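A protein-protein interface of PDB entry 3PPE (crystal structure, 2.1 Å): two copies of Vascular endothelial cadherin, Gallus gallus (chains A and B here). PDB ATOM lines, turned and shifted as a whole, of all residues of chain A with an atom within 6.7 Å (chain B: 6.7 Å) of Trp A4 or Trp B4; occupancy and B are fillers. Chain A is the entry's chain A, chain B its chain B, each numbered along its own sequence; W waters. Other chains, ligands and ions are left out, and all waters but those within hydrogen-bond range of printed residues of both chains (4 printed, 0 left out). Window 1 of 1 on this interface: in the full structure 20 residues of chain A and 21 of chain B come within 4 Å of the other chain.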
ATOM      1  N   TRP A   2     -21.125   9.321  -7.003  1.00  0.00           N
ATOM      2  CA  TRP A   2     -20.857   9.848  -5.652  1.00  0.00           C
ATOM      3  C   TRP A   2     -21.836  10.963  -5.343  1.00  0.00           C
ATOM      4  O   TRP A   2     -22.040  11.862  -6.145  1.00  0.00           O
ATOM      5  CB  TRP A   2     -19.412  10.336  -5.502  1.00  0.00           C
ATOM      6  CG  TRP A   2     -18.431   9.215  -5.626  1.00  0.00           C
ATOM      7  CD1 TRP A   2     -17.686   8.890  -6.737  1.00  0.00           C
ATOM      8  CD2 TRP A   2     -18.091   8.248  -4.622  1.00  0.00           C
ATOM      9  NE1 TRP A   2     -16.910   7.783  -6.476  1.00  0.00           N
ATOM     10  CE2 TRP A   2     -17.138   7.367  -5.192  1.00  0.00           C
ATOM     11  CE3 TRP A   2     -18.482   8.048  -3.289  1.00  0.00           C
ATOM     12  CZ2 TRP A   2     -16.574   6.306  -4.472  1.00  0.00           C
ATOM     13  CZ3 TRP A   2     -17.923   6.993  -2.587  1.00  0.00           C
ATOM     14  CH2 TRP A   2     -17.001   6.127  -3.185  1.00  0.00           C
ATOM     15  N   ILE A   3     -22.470  10.871  -4.212  1.00  0.00           N
ATOM     16  CA  ILE A   3     -23.402  11.897  -3.761  1.00  0.00           C
ATOM     17  C   ILE A   3     -22.809  12.722  -2.624  1.00  0.00           C
ATOM     18  O   ILE A   3     -22.482  12.170  -1.540  1.00  0.00           O
ATOM     19  CB  ILE A   3     -24.731  11.260  -3.313  1.00  0.00           C
ATOM     20  CG1 ILE A   3     -25.421  10.577  -4.496  1.00  0.00           C
ATOM     21  CG2 ILE A   3     -25.641  12.309  -2.693  1.00  0.00           C
ATOM     22  CD1 ILE A   3     -26.609   9.728  -4.102  1.00  0.00           C
ATOM     23  N   TRP A   4     -22.412  13.952  -2.884  1.00  0.00           N
ATOM     24  CA  TRP A   4     -21.714  14.771  -1.902  1.00  0.00           C
ATOM     25  C   TRP A   4     -22.604  15.902  -1.329  1.00  0.00           C
ATOM     26  O   TRP A   4     -22.305  16.429  -0.273  1.00  0.00           O
ATOM     27  CB  TRP A   4     -20.439  15.355  -2.524  1.00  0.00           C
ATOM     28  CG  TRP A   4     -19.309  14.379  -2.666  1.00  0.00           C
ATOM     29  CD1 TRP A   4     -18.808  13.864  -3.840  1.00  0.00           C
ATOM     30  CD2 TRP A   4     -18.510  13.821  -1.607  1.00  0.00           C
ATOM     31  NE1 TRP A   4     -17.752  13.012  -3.563  1.00  0.00           N
ATOM     32  CE2 TRP A   4     -17.558  12.962  -2.206  1.00  0.00           C
ATOM     33  CE3 TRP A   4     -18.510  13.959  -0.210  1.00  0.00           C
ATOM     34  CZ2 TRP A   4     -16.612  12.243  -1.458  1.00  0.00           C
ATOM     35  CZ3 TRP A   4     -17.559  13.232   0.535  1.00  0.00           C
ATOM     36  CH2 TRP A   4     -16.638  12.388  -0.103  1.00  0.00           C
ATOM     37  N   ASN A   5     -23.679  16.267  -2.022  1.00  0.00           N
ATOM     38  CA  ASN A   5     -24.587  17.336  -1.539  1.00  0.00           C
ATOM     39  C   ASN A   5     -25.629  16.840  -0.540  1.00  0.00           C
ATOM     40  O   ASN A   5     -26.821  16.861  -0.799  1.00  0.00           O
ATOM     41  CB  ASN A   5     -25.246  18.109  -2.693  1.00  0.00           C
ATOM     42  CG  ASN A   5     -26.106  17.225  -3.574  1.00  0.00           C
ATOM     43  OD1 ASN A   5     -25.804  16.032  -3.792  1.00  0.00           O
ATOM     44  ND2 ASN A   5     -27.191  17.805  -4.105  1.00  0.00           N
ATOM     45  N   ARG A   6     -25.133  16.388   0.599  1.00  0.00           N
ATOM     46  CA  ARG A   6     -25.901  15.736   1.624  1.00  0.00           C
ATOM     47  C   ARG A   6     -25.326  16.128   2.988  1.00  0.00           C
ATOM     48  O   ARG A   6     -24.115  16.306   3.133  1.00  0.00           O
ATOM     49  CB  ARG A   6     -25.747  14.219   1.518  1.00  0.00           C
ATOM     50  CG  ARG A   6     -26.361  13.564   0.305  1.00  0.00           C
ATOM     51  CD  ARG A   6     -27.884  13.402   0.453  1.00  0.00           C
ATOM     52  NE  ARG A   6     -28.494  12.799  -0.730  1.00  0.00           N
ATOM     53  CZ  ARG A   6     -28.786  13.447  -1.866  1.00  0.00           C
ATOM     54  NH1 ARG A   6     -28.515  14.749  -2.004  1.00  0.00           N
ATOM     55  NH2 ARG A   6     -29.359  12.775  -2.878  1.00  0.00           N
ATOM     56  N   MET A   7     -26.212  16.229   3.972  1.00  0.00           N
ATOM     57  CA  MET A   7     -25.818  16.312   5.373  1.00  0.00           C
ATOM     58  C   MET A   7     -26.589  15.200   6.073  1.00  0.00           C
ATOM     59  O   MET A   7     -27.620  14.752   5.578  1.00  0.00           O
ATOM     60  CB  MET A   7     -26.194  17.673   5.979  1.00  0.00           C
ATOM     61  CG  MET A   7     -25.524  18.870   5.287  1.00  0.00           C
ATOM     62  SD  MET A   7     -25.807  20.385   6.168  1.00  0.00           S
ATOM     63  CE  MET A   7     -25.020  21.534   5.039  1.00  0.00           C
ATOM     64  N   LYS A  23     -22.167  21.425   7.422  1.00  0.00           N
ATOM     65  CA  LYS A  23     -21.641  22.747   7.082  1.00  0.00           C
ATOM     66  C   LYS A  23     -21.685  23.022   5.607  1.00  0.00           C
ATOM     67  O   LYS A  23     -21.272  22.200   4.817  1.00  0.00           O
ATOM     68  CB  LYS A  23     -20.212  22.928   7.651  1.00  0.00           C
ATOM     69  CG  LYS A  23     -19.646  24.348   7.516  1.00  0.00           C
ATOM     70  CD  LYS A  23     -18.126  24.350   7.676  1.00  0.00           C
ATOM     71  CE  LYS A  23     -17.496  25.690   7.215  1.00  0.00           C
ATOM     72  NZ  LYS A  23     -17.756  26.196   5.777  1.00  0.00           N
ATOM     73  N   LEU A  24     -22.189  24.194   5.242  1.00  0.00           N
ATOM     74  CA  LEU A  24     -22.140  24.654   3.865  1.00  0.00           C
ATOM     75  C   LEU A  24     -20.802  25.289   3.567  1.00  0.00           C
ATOM     76  O   LEU A  24     -20.242  25.943   4.435  1.00  0.00           O
ATOM     77  CB  LEU A  24     -23.233  25.710   3.632  1.00  0.00           C
ATOM     78  CG  LEU A  24     -24.694  25.234   3.748  1.00  0.00           C
ATOM     79  CD1 LEU A  24     -25.596  26.487   3.692  1.00  0.00           C
ATOM     80  CD2 LEU A  24     -24.983  24.270   2.594  1.00  0.00           C
ATOM     81  N   THR A  25     -20.306  25.123   2.340  1.00  0.00           N
ATOM     82  CA  THR A  25     -19.114  25.864   1.901  1.00  0.00           C
ATOM     83  C   THR A  25     -19.263  26.389   0.474  1.00  0.00           C
ATOM     84  O   THR A  25     -19.433  25.617  -0.449  1.00  0.00           O
ATOM     85  CB  THR A  25     -17.820  25.016   2.000  1.00  0.00           C
ATOM     86  OG1 THR A  25     -17.670  24.492   3.326  1.00  0.00           O
ATOM     87  CG2 THR A  25     -16.569  25.872   1.657  1.00  0.00           C
ATOM     88  N   ALA A  73     -29.313  26.079  -0.728  1.00  0.00           N
ATOM     89  CA  ALA A  73     -28.381  27.002  -0.128  1.00  0.00           C
ATOM     90  C   ALA A  73     -28.098  28.188  -1.058  1.00  0.00           C
ATOM     91  O   ALA A  73     -28.055  28.037  -2.275  1.00  0.00           O
ATOM     92  CB  ALA A  73     -27.085  26.255   0.242  1.00  0.00           C
ATOM     93  N   SER A  88     -27.813  26.177  -4.433  1.00  0.00           N
ATOM     94  CA  SER A  88     -27.328  24.792  -4.472  1.00  0.00           C
ATOM     95  C   SER A  88     -28.289  23.919  -3.668  1.00  0.00           C
ATOM     96  O   SER A  88     -28.441  24.108  -2.462  1.00  0.00           O
ATOM     97  CB  SER A  88     -25.909  24.708  -3.899  1.00  0.00           C
ATOM     98  OG  SER A  88     -25.439  23.383  -3.922  1.00  0.00           O
ATOM     99  N   LYS A  89     -28.976  23.010  -4.357  1.00  0.00           N
ATOM    100  CA  LYS A  89     -29.847  22.037  -3.698  1.00  0.00           C
ATOM    101  C   LYS A  89     -29.065  20.966  -2.928  1.00  0.00           C
ATOM    102  O   LYS A  89     -28.063  20.444  -3.395  1.00  0.00           O
ATOM    103  CB  LYS A  89     -30.728  21.319  -4.737  1.00  0.00           C
ATOM    104  CG  LYS A  89     -31.776  22.182  -5.438  1.00  0.00           C
ATOM    105  CD  LYS A  89     -32.695  21.282  -6.320  1.00  0.00           C
ATOM    106  CE  LYS A  89     -32.269  21.217  -7.795  1.00  0.00           C
ATOM    107  NZ  LYS A  89     -33.146  22.034  -8.757  1.00  0.00           N
ATOM    108  N   PHE A  90     -29.587  20.579  -1.764  1.00  0.00           N
ATOM    109  CA  PHE A  90     -28.970  19.537  -0.971  1.00  0.00           C
ATOM    110  C   PHE A  90     -30.039  18.847  -0.144  1.00  0.00           C
ATOM    111  O   PHE A  90     -31.177  19.340  -0.017  1.00  0.00           O
ATOM    112  CB  PHE A  90     -27.785  20.076  -0.120  1.00  0.00           C
ATOM    113  CG  PHE A  90     -28.180  21.010   1.018  1.00  0.00           C
ATOM    114  CD1 PHE A  90     -28.476  22.352   0.778  1.00  0.00           C
ATOM    115  CD2 PHE A  90     -28.218  20.535   2.326  1.00  0.00           C
ATOM    116  CE1 PHE A  90     -28.837  23.218   1.827  1.00  0.00           C
ATOM    117  CE2 PHE A  90     -28.565  21.364   3.381  1.00  0.00           C
ATOM    118  CZ  PHE A  90     -28.897  22.714   3.144  1.00  0.00           C
ATOM    119  N   ILE A  91     -29.682  17.703   0.423  1.00  0.00           N
ATOM    120  CA  ILE A  91     -30.626  16.979   1.270  1.00  0.00           C
ATOM    121  C   ILE A  91     -29.992  16.782   2.636  1.00  0.00           C
ATOM    122  O   ILE A  91     -28.822  16.423   2.740  1.00  0.00           O
ATOM    123  CB  ILE A  91     -31.057  15.626   0.611  1.00  0.00           C
ATOM    124  CG1 ILE A  91     -31.948  15.923  -0.615  1.00  0.00           C
ATOM    125  CG2 ILE A  91     -31.753  14.700   1.635  1.00  0.00           C
ATOM    126  CD1 ILE A  91     -32.251  14.698  -1.603  1.00  0.00           C
ATOM    127  N   TRP B   2     -19.755  26.038  -5.062  1.00  0.00           N
ATOM    128  CA  TRP B   2     -20.096  25.334  -3.830  1.00  0.00           C
ATOM    129  C   TRP B   2     -19.184  24.143  -3.702  1.00  0.00           C
ATOM    130  O   TRP B   2     -18.997  23.434  -4.677  1.00  0.00           O
ATOM    131  CB  TRP B   2     -21.542  24.872  -3.894  1.00  0.00           C
ATOM    132  CG  TRP B   2     -22.542  26.041  -3.805  1.00  0.00           C
ATOM    133  CD1 TRP B   2     -23.196  26.662  -4.864  1.00  0.00           C
ATOM    134  CD2 TRP B   2     -23.009  26.690  -2.607  1.00  0.00           C
ATOM    135  NE1 TRP B   2     -24.027  27.658  -4.386  1.00  0.00           N
ATOM    136  CE2 TRP B   2     -23.935  27.696  -3.012  1.00  0.00           C
ATOM    137  CE3 TRP B   2     -22.735  26.530  -1.236  1.00  0.00           C
ATOM    138  CZ2 TRP B   2     -24.580  28.532  -2.089  1.00  0.00           C
ATOM    139  CZ3 TRP B   2     -23.394  27.368  -0.307  1.00  0.00           C
ATOM    140  CH2 TRP B   2     -24.295  28.351  -0.746  1.00  0.00           C
ATOM    141  N   ILE B   3     -18.597  23.926  -2.529  1.00  0.00           N
ATOM    142  CA  ILE B   3     -17.701  22.802  -2.287  1.00  0.00           C
ATOM    143  C   ILE B   3     -18.365  21.745  -1.409  1.00  0.00           C
ATOM    144  O   ILE B   3     -18.630  21.969  -0.198  1.00  0.00           O
ATOM    145  CB  ILE B   3     -16.393  23.285  -1.635  1.00  0.00           C
ATOM    146  CG1 ILE B   3     -15.634  24.212  -2.586  1.00  0.00           C
ATOM    147  CG2 ILE B   3     -15.529  22.101  -1.235  1.00  0.00           C
ATOM    148  CD1 ILE B   3     -14.461  24.919  -1.944  1.00  0.00           C
ATOM    149  N   TRP B   4     -18.776  20.652  -2.023  1.00  0.00           N
ATOM    150  CA  TRP B   4     -19.529  19.634  -1.335  1.00  0.00           C
ATOM    151  C   TRP B   4     -18.691  18.418  -0.921  1.00  0.00           C
ATOM    152  O   TRP B   4     -19.101  17.682  -0.020  1.00  0.00           O
ATOM    153  CB  TRP B   4     -20.738  19.215  -2.178  1.00  0.00           C
ATOM    154  CG  TRP B   4     -21.874  20.201  -2.101  1.00  0.00           C
ATOM    155  CD1 TRP B   4     -22.326  21.019  -3.094  1.00  0.00           C
ATOM    156  CD2 TRP B   4     -22.695  20.463  -0.954  1.00  0.00           C
ATOM    157  NE1 TRP B   4     -23.399  21.748  -2.646  1.00  0.00           N
ATOM    158  CE2 TRP B   4     -23.638  21.436  -1.331  1.00  0.00           C
ATOM    159  CE3 TRP B   4     -22.737  19.944   0.347  1.00  0.00           C
ATOM    160  CZ2 TRP B   4     -24.606  21.925  -0.452  1.00  0.00           C
ATOM    161  CZ3 TRP B   4     -23.713  20.429   1.232  1.00  0.00           C
ATOM    162  CH2 TRP B   4     -24.637  21.402   0.814  1.00  0.00           C
ATOM    163  N   ASN B   5     -17.542  18.208  -1.567  1.00  0.00           N
ATOM    164  CA  ASN B   5     -16.695  17.001  -1.291  1.00  0.00           C
ATOM    165  C   ASN B   5     -15.750  17.257  -0.121  1.00  0.00           C
ATOM    166  O   ASN B   5     -14.527  17.284  -0.259  1.00  0.00           O
ATOM    167  CB  ASN B   5     -15.945  16.528  -2.554  1.00  0.00           C
ATOM    168  CG  ASN B   5     -14.993  17.585  -3.111  1.00  0.00           C
ATOM    169  OD1 ASN B   5     -15.256  18.786  -3.027  1.00  0.00           O
ATOM    170  ND2 ASN B   5     -13.885  17.133  -3.694  1.00  0.00           N
ATOM    171  N   ARG B   6     -16.386  17.516   1.024  1.00  0.00           N
ATOM    172  CA  ARG B   6     -15.740  17.860   2.266  1.00  0.00           C
ATOM    173  C   ARG B   6     -16.404  17.199   3.462  1.00  0.00           C
ATOM    174  O   ARG B   6     -17.624  17.062   3.532  1.00  0.00           O
ATOM    175  CB  ARG B   6     -15.858  19.355   2.524  1.00  0.00           C
ATOM    176  CG  ARG B   6     -15.169  20.248   1.561  1.00  0.00           C
ATOM    177  CD  ARG B   6     -13.720  20.508   1.943  1.00  0.00           C
ATOM    178  NE  ARG B   6     -13.012  20.473   0.676  1.00  0.00           N
ATOM    179  CZ  ARG B   6     -12.520  21.514   0.019  1.00  0.00           C
ATOM    180  NH1 ARG B   6     -12.602  22.731   0.555  1.00  0.00           N
ATOM    181  NH2 ARG B   6     -11.937  21.321  -1.182  1.00  0.00           N
ATOM    182  N   MET B   7     -15.586  16.885   4.453  1.00  0.00           N
ATOM    183  CA  MET B   7     -16.067  16.506   5.755  1.00  0.00           C
ATOM    184  C   MET B   7     -15.384  17.447   6.717  1.00  0.00           C
ATOM    185  O   MET B   7     -14.328  18.035   6.388  1.00  0.00           O
ATOM    186  CB  MET B   7     -15.678  15.045   6.066  1.00  0.00           C
ATOM    187  CG  MET B   7     -16.276  14.043   5.107  1.00  0.00           C
ATOM    188  SD  MET B   7     -16.022  12.343   5.593  1.00  0.00           S
ATOM    189  CE  MET B   7     -16.871  11.530   4.252  1.00  0.00           C
ATOM    190  N   LYS B  23     -19.783  11.001   6.304  1.00  0.00           N
ATOM    191  CA  LYS B  23     -20.304   9.797   5.655  1.00  0.00           C
ATOM    192  C   LYS B  23     -20.115   9.881   4.144  1.00  0.00           C
ATOM    193  O   LYS B  23     -20.457  10.889   3.529  1.00  0.00           O
ATOM    194  CB  LYS B  23     -21.804   9.579   5.974  1.00  0.00           C
ATOM    195  CG  LYS B  23     -22.370   8.234   5.418  1.00  0.00           C
ATOM    196  CD  LYS B  23     -23.913   8.272   5.277  1.00  0.00           C
ATOM    197  CE  LYS B  23     -24.497   7.076   4.487  1.00  0.00           C
ATOM    198  NZ  LYS B  23     -23.919   6.814   3.084  1.00  0.00           N
ATOM    199  N   LEU B  24     -19.571   8.815   3.568  1.00  0.00           N
ATOM    200  CA  LEU B  24     -19.489   8.669   2.121  1.00  0.00           C
ATOM    201  C   LEU B  24     -20.783   8.102   1.544  1.00  0.00           C
ATOM    202  O   LEU B  24     -21.361   7.194   2.141  1.00  0.00           O
ATOM    203  CB  LEU B  24     -18.346   7.717   1.763  1.00  0.00           C
ATOM    204  CG  LEU B  24     -16.920   8.062   2.173  1.00  0.00           C
ATOM    205  CD1 LEU B  24     -16.032   6.868   1.928  1.00  0.00           C
ATOM    206  CD2 LEU B  24     -16.455   9.266   1.368  1.00  0.00           C
ATOM    207  N   THR B  25     -21.211   8.593   0.376  1.00  0.00           N
ATOM    208  CA  THR B  25     -22.386   8.032  -0.340  1.00  0.00           C
ATOM    209  C   THR B  25     -22.149   7.825  -1.840  1.00  0.00           C
ATOM    210  O   THR B  25     -21.827   8.763  -2.571  1.00  0.00           O
ATOM    211  CB  THR B  25     -23.677   8.882  -0.136  1.00  0.00           C
ATOM    212  OG1 THR B  25     -23.986   8.937   1.265  1.00  0.00           O
ATOM    213  CG2 THR B  25     -24.889   8.260  -0.891  1.00  0.00           C
ATOM    214  N   ALA B  73     -11.914   8.233  -1.840  1.00  0.00           N
ATOM    215  CA  ALA B  73     -12.859   7.152  -1.548  1.00  0.00           C
ATOM    216  C   ALA B  73     -13.021   6.229  -2.771  1.00  0.00           C
ATOM    217  O   ALA B  73     -13.045   6.698  -3.919  1.00  0.00           O
ATOM    218  CB  ALA B  73     -14.233   7.751  -1.217  1.00  0.00           C
ATOM    219  N   SER B  88     -13.271   8.947  -5.775  1.00  0.00           N
ATOM    220  CA  SER B  88     -13.665  10.338  -5.548  1.00  0.00           C
ATOM    221  C   SER B  88     -12.736  10.978  -4.496  1.00  0.00           C
ATOM    222  O   SER B  88     -12.671  10.494  -3.366  1.00  0.00           O
ATOM    223  CB  SER B  88     -15.109  10.382  -5.058  1.00  0.00           C
ATOM    224  OG  SER B  88     -15.589  11.721  -4.942  1.00  0.00           O
ATOM    225  N   LYS B  89     -12.014  12.027  -4.889  1.00  0.00           N
ATOM    226  CA  LYS B  89     -11.206  12.844  -3.961  1.00  0.00           C
ATOM    227  C   LYS B  89     -12.051  13.736  -3.027  1.00  0.00           C
ATOM    228  O   LYS B  89     -13.067  14.278  -3.424  1.00  0.00           O
ATOM    229  CB  LYS B  89     -10.238  13.727  -4.741  1.00  0.00           C
ATOM    230  CG  LYS B  89      -9.003  13.019  -5.310  1.00  0.00           C
ATOM    231  CD  LYS B  89      -8.062  14.083  -5.921  1.00  0.00           C
ATOM    232  CE  LYS B  89      -6.576  13.836  -5.578  1.00  0.00           C
ATOM    233  NZ  LYS B  89      -5.813  13.157  -6.696  1.00  0.00           N
ATOM    234  N   PHE B  90     -11.614  13.864  -1.777  1.00  0.00           N
ATOM    235  CA  PHE B  90     -12.300  14.688  -0.782  1.00  0.00           C
ATOM    236  C   PHE B  90     -11.311  15.146   0.296  1.00  0.00           C
ATOM    237  O   PHE B  90     -10.186  14.596   0.404  1.00  0.00           O
ATOM    238  CB  PHE B  90     -13.564  13.968  -0.197  1.00  0.00           C
ATOM    239  CG  PHE B  90     -13.261  12.798   0.720  1.00  0.00           C
ATOM    240  CD1 PHE B  90     -12.897  11.539   0.196  1.00  0.00           C
ATOM    241  CD2 PHE B  90     -13.355  12.952   2.116  1.00  0.00           C
ATOM    242  CE1 PHE B  90     -12.627  10.470   1.040  1.00  0.00           C
ATOM    243  CE2 PHE B  90     -13.102  11.889   2.969  1.00  0.00           C
ATOM    244  CZ  PHE B  90     -12.730  10.632   2.428  1.00  0.00           C
ATOM    245  N   ILE B  91     -11.708  16.168   1.063  1.00  0.00           N
ATOM    246  CA  ILE B  91     -10.868  16.705   2.096  1.00  0.00           C
ATOM    247  C   ILE B  91     -11.592  16.643   3.422  1.00  0.00           C
ATOM    248  O   ILE B  91     -12.787  16.995   3.534  1.00  0.00           O
ATOM    249  CB  ILE B  91     -10.323  18.155   1.794  1.00  0.00           C
ATOM    250  CG1 ILE B  91      -9.308  18.115   0.632  1.00  0.00           C
ATOM    251  CG2 ILE B  91      -9.585  18.710   3.037  1.00  0.00           C
ATOM    252  CD1 ILE B  91      -8.863  19.471   0.076  1.00  0.00           C
HETATM  253  O   HOH W   1     -18.858  21.921   2.977  1.00  0.00           O
HETATM  254  O   HOH W   2     -22.587  11.824   1.513  1.00  0.00           O
HETATM  255  O   HOH W   3     -19.997  10.757  -0.894  1.00  0.00           O
HETATM  256  O   HOH W   4     -21.458  23.288   0.712  1.00  0.00           O
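Thr B25 touches Trp A2.
Trp A2 touches Ala B73 (CZ2 to O, 3.6 Å).
Trp A2 touches Ser B88.
CD2 of Trp A4 touches CA of Asn B5 (3.7 Å).
CH2 of Trp A4 touches CD2 of Leu B24 (3.5 Å).
Leu A24 touches Trp B4 (CD2 to CH2, 3.4 Å).
CA of Trp B2 touches O of Thr A25, 3.5 Å away.
Trp B2 touches Ala A73 (CZ2 to O, 3.5 Å).
Ser A88 touches Trp B2.
Phe A90 touches Trp B4 (CB to CH2, 3.5 Å).
The side-chain amide oxygen of Asn A5 sits at hydrogen-bond distance from the guanidinium group of Arg A6 (3.5 Å).
The side-chain amino group of Lys A23 sits at hydrogen-bond distance from the side-chain hydroxyl of Thr A25 (3.0 Å).
ND2 of Asn B5 is in hydrogen-bond range of O of Lys B89 (3.0 Å).
The backbone carbonyl oxygen (O) of Asn B5 lies within hydrogen-bond range of the backbone NH (N) of Ile B91, 3.3 Å away.
NZ of Lys B23 sits at hydrogen-bond distance from OG1 of Thr B25 (2.8 Å).
The backbone NH (N) of Ala B73 lies within hydrogen-bond range of the backbone carbonyl oxygen (O) of Ser B88.
Of the 14 printed residues of chain B, 9 touch a printed residue of chain A.
Printed residues of chain B that touch a printed residue of chain A: Trp B2, Ile B3, Trp B4, Asn B5, Leu B24, Thr B25, Ala B73, Ser B88 and Phe B90.
Hydrophobic or aromatic side chains of chain B within 4 Å of the printed part of chain A: Trp B2, Trp B4, Leu B24, Ala B73 and Phe B90.
Hydrophobic or aromatic side chains of chain A within 4 Å of the printed part of chain B: Trp A2, Ile A3, Trp A4, Leu A24, Ala A73 and Phe A90.
Along chain A the printed residues that touch a printed residue of chain B span positions 2 to 90.
Among the printed residues, 17 pairs touch across the chains.
Among the printed residues, no Asp or Glu carboxylate lies within 4 Å of a Lys or Arg side-chain nitrogen of the other chain.
Trp A4 touches five residues of chain B.
Printed residues of chain B within 4 Å of Asn A5: Trp B4 (3.7 Å).
Lys A23 touches none of the printed residues of chain B.
Of the printed residues of chain B, Leu A24 touches Trp B4 (3.4 Å).
Of the printed residues of chain B, Ser A88 touches Trp B2 (3.5 Å) and Trp B4 (2.9 Å).
Printed residues of chain A within 4 Å of Trp B2: Thr A25, Ala A73 and Ser A88.
Trp B4 touches five residues of chain A.
Met B7 touches none of the printed residues of chain A.
Printed residues of chain A within 4 Å of Leu B24: Trp A4.
The nearest residue of chain B that does not touch Trp A4 is Met B7 (4.1 Å).
The nearest residue of chain A that does not touch Trp B4 is Met A7 (4.2 Å).
Trp A2 touches Thr B25, and with the chains exchanged Thr A25 touches Trp B2.
Trp A2 touches Ala B73, and with the chains exchanged Ala A73 touches Trp B2.
Trp A4 touches Ser B88, and with the chains exchanged Ser A88 touches Trp B4.
Trp A4 touches Phe B90, and with the chains exchanged Phe A90 touches Trp B4.
Of the 17 pairs that touch across the chains among the printed residues, 17 have their exchanged pair printed and touching as well.
The backbone carbonyl oxygen (O) of Thr B25 sits at hydrogen-bond distance from the backbone NH (N) of Ile A3 (2.7 Å).
The side-chain hydroxyl of Ser B88 is in hydrogen-bond range of the indole nitrogen of Trp A4, at 2.9 Å.
O of Thr A25 lies within hydrogen-bond range of N of Ile B3 (2.8 Å).
OG of Ser A88 lies within hydrogen-bond range of NE1 of Trp B4 (2.9 Å).
The backbone carbonyl oxygen of Trp A4 sits close to the backbone carbonyl oxygen of Trp B4.
Water W4 bridges N of Thr A25 (2.7 Å) and O of Ile B3 (3.3 Å).
Water W3 bridges the backbone NH of Thr B25 and the backbone carbonyl oxygen of Ile A3.
Water W1 lies within hydrogen-bond range of the side-chain hydroxyl of Thr A25 (2.9 Å), the backbone carbonyl oxygen of Lys A23 (3.0 Å) and the backbone carbonyl oxygen of Ile B3 (3.2 Å).
Water W2 lies within hydrogen-bond range of the backbone carbonyl oxygen of Ile A3, the backbone carbonyl oxygen of Lys B23 and the side-chain hydroxyl of Thr B25.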
